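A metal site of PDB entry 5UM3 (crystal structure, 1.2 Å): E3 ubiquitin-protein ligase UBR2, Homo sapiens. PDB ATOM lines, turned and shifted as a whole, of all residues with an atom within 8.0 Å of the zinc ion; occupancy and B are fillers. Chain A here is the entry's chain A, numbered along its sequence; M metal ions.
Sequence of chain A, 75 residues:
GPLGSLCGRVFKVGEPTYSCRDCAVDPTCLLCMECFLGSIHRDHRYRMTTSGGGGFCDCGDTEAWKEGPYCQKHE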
ATOM      1  N   SER A  19      14.820 -26.960  15.792  1.00  0.00           N
ATOM      2  CA  SER A  19      14.345 -27.972  14.853  1.00  0.00           C
ATOM      3  C   SER A  19      12.935 -27.583  14.417  1.00  0.00           C
ATOM      4  O   SER A  19      12.039 -27.447  15.263  1.00  0.00           O
ATOM      5  CB  SER A  19      14.299 -29.354  15.518  1.00  0.00           C
ATOM      6  OG  SER A  19      13.504 -30.268  14.766  1.00  0.00           O
ATOM      7  N   CYS A  20      12.731 -27.385  13.124  1.00  0.00           N
ATOM      8  CA  CYS A  20      11.375 -27.198  12.631  1.00  0.00           C
ATOM      9  C   CYS A  20      10.755 -28.570  12.431  1.00  0.00           C
ATOM     10  O   CYS A  20      11.206 -29.340  11.588  1.00  0.00           O
ATOM     11  CB  CYS A  20      11.351 -26.434  11.308  1.00  0.00           C
ATOM     12  SG  CYS A  20       9.585 -26.180  10.918  1.00  0.00           S
ATOM     13  N   ARG A  21       9.719 -28.876  13.218  1.00  0.00           N
ATOM     14  CA  ARG A  21       9.086 -30.188  13.096  1.00  0.00           C
ATOM     15  C   ARG A  21       8.344 -30.319  11.781  1.00  0.00           C
ATOM     16  O   ARG A  21       8.180 -31.430  11.271  1.00  0.00           O
ATOM     17  CB  ARG A  21       8.132 -30.432  14.264  1.00  0.00           C
ATOM     18  CG  ARG A  21       8.720 -30.106  15.612  1.00  0.00           C
ATOM     19  CD  ARG A  21      10.096 -30.749  15.817  1.00  0.00           C
ATOM     20  NE  ARG A  21      10.039 -32.204  15.899  1.00  0.00           N
ATOM     21  CZ  ARG A  21      11.090 -32.999  16.068  1.00  0.00           C
ATOM     22  NH1 ARG A  21      12.331 -32.491  16.131  1.00  0.00           N
ATOM     23  NH2 ARG A  21      10.895 -34.313  16.145  1.00  0.00           N
ATOM     24  N   ASP A  22       7.867 -29.207  11.218  1.00  0.00           N
ATOM     25  CA  ASP A  22       7.133 -29.254   9.964  1.00  0.00           C
ATOM     26  C   ASP A  22       8.069 -29.463   8.775  1.00  0.00           C
ATOM     27  O   ASP A  22       7.690 -30.136   7.812  1.00  0.00           O
ATOM     28  CB  ASP A  22       6.333 -27.962   9.773  1.00  0.00           C
ATOM     29  CG  ASP A  22       5.258 -27.763  10.845  1.00  0.00           C
ATOM     30  OD1 ASP A  22       5.062 -26.624  11.310  1.00  0.00           O
ATOM     31  OD2 ASP A  22       4.615 -28.769  11.236  1.00  0.00           O
ATOM     32  N   CYS A  23       9.296 -28.952   8.837  1.00  0.00           N
ATOM     33  CA  CYS A  23      10.159 -28.908   7.665  1.00  0.00           C
ATOM     34  C   CYS A  23      11.433 -29.733   7.764  1.00  0.00           C
ATOM     35  O   CYS A  23      12.024 -30.037   6.714  1.00  0.00           O
ATOM     36  CB  CYS A  23      10.538 -27.450   7.325  1.00  0.00           C
ATOM     37  SG  CYS A  23       9.080 -26.390   7.076  1.00  0.00           S
ATOM     38  N   ALA A  24      11.903 -30.093   8.946  1.00  0.00           N
ATOM     39  CA  ALA A  24      13.147 -30.849   9.047  1.00  0.00           C
ATOM     40  C   ALA A  24      13.004 -32.185   8.321  1.00  0.00           C
ATOM     41  O   ALA A  24      12.006 -32.893   8.463  1.00  0.00           O
ATOM     42  CB  ALA A  24      13.495 -31.112  10.510  1.00  0.00           C
ATOM     43  N   LEU A  31      18.751 -25.309  13.085  1.00  0.00           N
ATOM     44  CA  LEU A  31      19.053 -23.917  12.783  1.00  0.00           C
ATOM     45  C   LEU A  31      19.564 -23.194  14.020  1.00  0.00           C
ATOM     46  O   LEU A  31      19.122 -23.465  15.136  1.00  0.00           O
ATOM     47  CB  LEU A  31      17.804 -23.195  12.311  1.00  0.00           C
ATOM     48  CG  LEU A  31      17.196 -23.746  11.028  1.00  0.00           C
ATOM     49  CD1 LEU A  31      15.821 -23.163  10.779  1.00  0.00           C
ATOM     50  CD2 LEU A  31      18.106 -23.454   9.835  1.00  0.00           C
ATOM     51  N   PHE A  36      16.961 -19.192  12.412  1.00  0.00           N
ATOM     52  CA  PHE A  36      15.597 -19.582  12.720  1.00  0.00           C
ATOM     53  C   PHE A  36      14.668 -18.376  12.701  1.00  0.00           C
ATOM     54  O   PHE A  36      13.611 -18.402  12.048  1.00  0.00           O
ATOM     55  CB  PHE A  36      15.567 -20.265  14.082  1.00  0.00           C
ATOM     56  CG  PHE A  36      14.191 -20.588  14.562  1.00  0.00           C
ATOM     57  CD1 PHE A  36      13.442 -21.617  13.986  1.00  0.00           C
ATOM     58  CD2 PHE A  36      13.614 -19.846  15.589  1.00  0.00           C
ATOM     59  CE1 PHE A  36      12.169 -21.898  14.426  1.00  0.00           C
ATOM     60  CE2 PHE A  36      12.324 -20.129  16.040  1.00  0.00           C
ATOM     61  CZ  PHE A  36      11.613 -21.158  15.449  1.00  0.00           C
ATOM     62  N   SER A  39      13.728 -16.940   9.278  1.00  0.00           N
ATOM     63  CA  SER A  39      13.267 -17.972   8.358  1.00  0.00           C
ATOM     64  C   SER A  39      11.758 -18.132   8.484  1.00  0.00           C
ATOM     65  O   SER A  39      11.128 -17.638   9.416  1.00  0.00           O
ATOM     66  CB  SER A  39      13.938 -19.317   8.655  1.00  0.00           C
ATOM     67  OG  SER A  39      13.324 -19.928   9.772  1.00  0.00           O
ATOM     68  N   ILE A  40      11.162 -18.879   7.548  1.00  0.00           N
ATOM     69  CA  ILE A  40       9.739 -19.169   7.642  1.00  0.00           C
ATOM     70  C   ILE A  40       9.446 -20.028   8.857  1.00  0.00           C
ATOM     71  O   ILE A  40       8.296 -20.086   9.316  1.00  0.00           O
ATOM     72  CB  ILE A  40       9.186 -19.867   6.381  1.00  0.00           C
ATOM     73  CG1 ILE A  40       9.789 -21.265   6.212  1.00  0.00           C
ATOM     74  CG2 ILE A  40       9.461 -19.019   5.173  1.00  0.00           C
ATOM     75  CD1 ILE A  40       9.176 -22.060   5.066  1.00  0.00           C
ATOM     76  N   HIS A  41      10.445 -20.714   9.394  1.00  0.00           N
ATOM     77  CA  HIS A  41      10.193 -21.671  10.479  1.00  0.00           C
ATOM     78  C   HIS A  41       9.882 -20.993  11.800  1.00  0.00           C
ATOM     79  O   HIS A  41       9.393 -21.672  12.699  1.00  0.00           O
ATOM     80  CB  HIS A  41      11.380 -22.627  10.591  1.00  0.00           C
ATOM     81  CG  HIS A  41      11.830 -23.132   9.268  1.00  0.00           C
ATOM     82  ND1 HIS A  41      11.047 -23.990   8.506  1.00  0.00           N
ATOM     83  CD2 HIS A  41      12.894 -22.818   8.504  1.00  0.00           C
ATOM     84  CE1 HIS A  41      11.656 -24.214   7.349  1.00  0.00           C
ATOM     85  NE2 HIS A  41      12.774 -23.507   7.332  1.00  0.00           N
ATOM     86  N   ARG A  42      10.127 -19.685  11.921  1.00  0.00           N
ATOM     87  CA  ARG A  42       9.813 -18.974  13.154  1.00  0.00           C
ATOM     88  C   ARG A  42       8.344 -19.095  13.507  1.00  0.00           C
ATOM     89  O   ARG A  42       7.987 -19.016  14.691  1.00  0.00           O
ATOM     90  CB  ARG A  42      10.216 -17.507  13.012  1.00  0.00           C
ATOM     91  CG  ARG A  42       9.403 -16.714  11.995  1.00  0.00           C
ATOM     92  CD  ARG A  42      10.154 -15.450  11.532  1.00  0.00           C
ATOM     93  NE  ARG A  42       9.308 -14.503  10.811  1.00  0.00           N
ATOM     94  CZ  ARG A  42       8.874 -14.650   9.557  1.00  0.00           C
ATOM     95  NH1 ARG A  42       9.211 -15.726   8.861  1.00  0.00           N
ATOM     96  NH2 ARG A  42       8.109 -13.739   8.986  1.00  0.00           N
ATOM     97  N   ASP A  43       7.492 -19.293  12.505  1.00  0.00           N
ATOM     98  CA  ASP A  43       6.053 -19.389  12.690  1.00  0.00           C
ATOM     99  C   ASP A  43       5.542 -20.819  12.516  1.00  0.00           C
ATOM    100  O   ASP A  43       4.321 -21.033  12.435  1.00  0.00           O
ATOM    101  CB  ASP A  43       5.352 -18.446  11.717  1.00  0.00           C
ATOM    102  CG  ASP A  43       5.649 -16.984  12.009  1.00  0.00           C
ATOM    103  OD1 ASP A  43       5.830 -16.630  13.188  1.00  0.00           O
ATOM    104  OD2 ASP A  43       5.719 -16.184  11.046  1.00  0.00           O
ATOM    105  N   HIS A  44       6.442 -21.809  12.488  1.00  0.00           N
ATOM    106  CA  HIS A  44       6.077 -23.212  12.354  1.00  0.00           C
ATOM    107  C   HIS A  44       6.118 -23.905  13.712  1.00  0.00           C
ATOM    108  O   HIS A  44       6.446 -23.300  14.733  1.00  0.00           O
ATOM    109  CB  HIS A  44       7.018 -23.914  11.388  1.00  0.00           C
ATOM    110  CG  HIS A  44       6.854 -23.471   9.972  1.00  0.00           C
ATOM    111  ND1 HIS A  44       7.665 -23.919   8.958  1.00  0.00           N
ATOM    112  CD2 HIS A  44       5.966 -22.619   9.408  1.00  0.00           C
ATOM    113  CE1 HIS A  44       7.271 -23.364   7.828  1.00  0.00           C
ATOM    114  NE2 HIS A  44       6.246 -22.576   8.074  1.00  0.00           N
ATOM    115  N   ARG A  45       5.775 -25.185  13.701  1.00  0.00           N
ATOM    116  CA  ARG A  45       5.883 -26.029  14.886  1.00  0.00           C
ATOM    117  C   ARG A  45       7.348 -26.396  15.066  1.00  0.00           C
ATOM    118  O   ARG A  45       7.927 -27.057  14.197  1.00  0.00           O
ATOM    119  CB  ARG A  45       5.047 -27.282  14.687  1.00  0.00           C
ATOM    120  CG  ARG A  45       4.977 -28.200  15.884  1.00  0.00           C
ATOM    121  N   TYR A  46       7.959 -25.968  16.157  1.00  0.00           N
ATOM    122  CA  TYR A  46       9.390 -26.128  16.316  1.00  0.00           C
ATOM    123  C   TYR A  46       9.721 -26.583  17.726  1.00  0.00           C
ATOM    124  O   TYR A  46       8.906 -26.498  18.647  1.00  0.00           O
ATOM    125  CB  TYR A  46      10.140 -24.833  16.001  1.00  0.00           C
ATOM    126  CG  TYR A  46      10.007 -23.758  17.052  1.00  0.00           C
ATOM    127  CD1 TYR A  46       8.953 -22.852  17.019  1.00  0.00           C
ATOM    128  CD2 TYR A  46      10.939 -23.623  18.073  1.00  0.00           C
ATOM    129  CE1 TYR A  46       8.839 -21.854  17.980  1.00  0.00           C
ATOM    130  CE2 TYR A  46      10.838 -22.643  19.016  1.00  0.00           C
ATOM    131  CZ  TYR A  46       9.779 -21.764  18.973  1.00  0.00           C
ATOM    132  OH  TYR A  46       9.686 -20.778  19.926  1.00  0.00           O
ATOM    133  N   TRP A  65      15.848 -29.381   4.584  1.00  0.00           N
ATOM    134  CA  TRP A  65      14.573 -28.722   4.816  1.00  0.00           C
ATOM    135  C   TRP A  65      13.627 -29.021   3.660  1.00  0.00           C
ATOM    136  O   TRP A  65      13.996 -28.859   2.491  1.00  0.00           O
ATOM    137  CB  TRP A  65      14.773 -27.199   4.955  1.00  0.00           C
ATOM    138  CG  TRP A  65      15.808 -26.902   5.993  1.00  0.00           C
ATOM    139  CD1 TRP A  65      17.082 -26.466   5.772  1.00  0.00           C
ATOM    140  CD2 TRP A  65      15.690 -27.095   7.403  1.00  0.00           C
ATOM    141  NE1 TRP A  65      17.756 -26.365   6.963  1.00  0.00           N
ATOM    142  CE2 TRP A  65      16.920 -26.734   7.985  1.00  0.00           C
ATOM    143  CE3 TRP A  65      14.651 -27.516   8.242  1.00  0.00           C
ATOM    144  CZ2 TRP A  65      17.145 -26.807   9.364  1.00  0.00           C
ATOM    145  CZ3 TRP A  65      14.873 -27.580   9.600  1.00  0.00           C
ATOM    146  CH2 TRP A  65      16.105 -27.239  10.146  1.00  0.00           C
ATOM    147  N   LYS A  66      12.412 -29.437   4.006  1.00  0.00           N
ATOM    148  CA  LYS A  66      11.380 -29.661   3.002  1.00  0.00           C
ATOM    149  C   LYS A  66      10.892 -28.349   2.398  1.00  0.00           C
ATOM    150  O   LYS A  66      10.449 -28.327   1.245  1.00  0.00           O
ATOM    151  CB  LYS A  66      10.219 -30.436   3.627  1.00  0.00           C
ATOM    152  CG  LYS A  66      10.594 -31.845   4.015  1.00  0.00           C
ATOM    153  CD  LYS A  66       9.423 -32.604   4.628  1.00  0.00           C
ATOM    154  CE  LYS A  66       9.196 -32.209   6.068  1.00  0.00           C
ATOM    155  NZ  LYS A  66       8.104 -33.004   6.686  1.00  0.00           N
ATOM    156  N   GLU A  67      10.946 -27.265   3.172  1.00  0.00           N
ATOM    157  CA  GLU A  67      10.539 -25.933   2.744  1.00  0.00           C
ATOM    158  C   GLU A  67      11.453 -24.923   3.418  1.00  0.00           C
ATOM    159  O   GLU A  67      12.004 -25.187   4.482  1.00  0.00           O
ATOM    160  CB  GLU A  67       9.087 -25.624   3.148  1.00  0.00           C
ATOM    161  CG  GLU A  67       8.083 -26.670   2.694  1.00  0.00           C
ATOM    162  CD  GLU A  67       7.844 -26.679   1.193  1.00  0.00           C
ATOM    163  OE1 GLU A  67       8.312 -25.749   0.495  1.00  0.00           O
ATOM    164  OE2 GLU A  67       7.157 -27.617   0.721  1.00  0.00           O
ATOM    165  N   GLY A  68      11.625 -23.755   2.783  1.00  0.00           N
ATOM    166  CA  GLY A  68      12.366 -22.655   3.375  1.00  0.00           C
ATOM    167  C   GLY A  68      13.776 -22.989   3.837  1.00  0.00           C
ATOM    168  O   GLY A  68      14.146 -22.762   4.990  1.00  0.00           O
HETATM  169 ZN    ZN M   1       9.346 -25.083   8.930  1.00  0.00          ZN
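The zinc ion is bound by ND1 of His 44, ND1 of His 41, SG of Cys 20 and SG of Cys 23.
Four residues have an atom within 4 Å of the zinc ion: Cys 20, Cys 23, His 41 and His 44.
A ring nitrogen (NE2) of His 44 sits close to the backbone carbonyl oxygen (O) of Ile 40, 3.5 Å away. A ring nitrogen (NE2) of His 41 sits close to the backbone carbonyl oxygen (O) of Glu 67 (3.4 Å). N of His 41 lies within hydrogen-bond range of OG of Ser 39 (3.0 Å). The backbone carbonyl oxygen of Gly 68 is in hydrogen-bond range of a ring nitrogen (NE2) of His 41, 2.8 Å away. The side-chain sulfur of Cys 20 lies close to the backbone NH of Asp 22 (3.5 Å). The backbone carbonyl oxygen (O) of Arg 45 lies close to the side-chain sulfur (SG) of Cys 20 (3.8 Å). The backbone NH (N) of Lys 66 sits at hydrogen-bond distance from the backbone carbonyl oxygen (O) of Cys 23 (2.8 Å).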
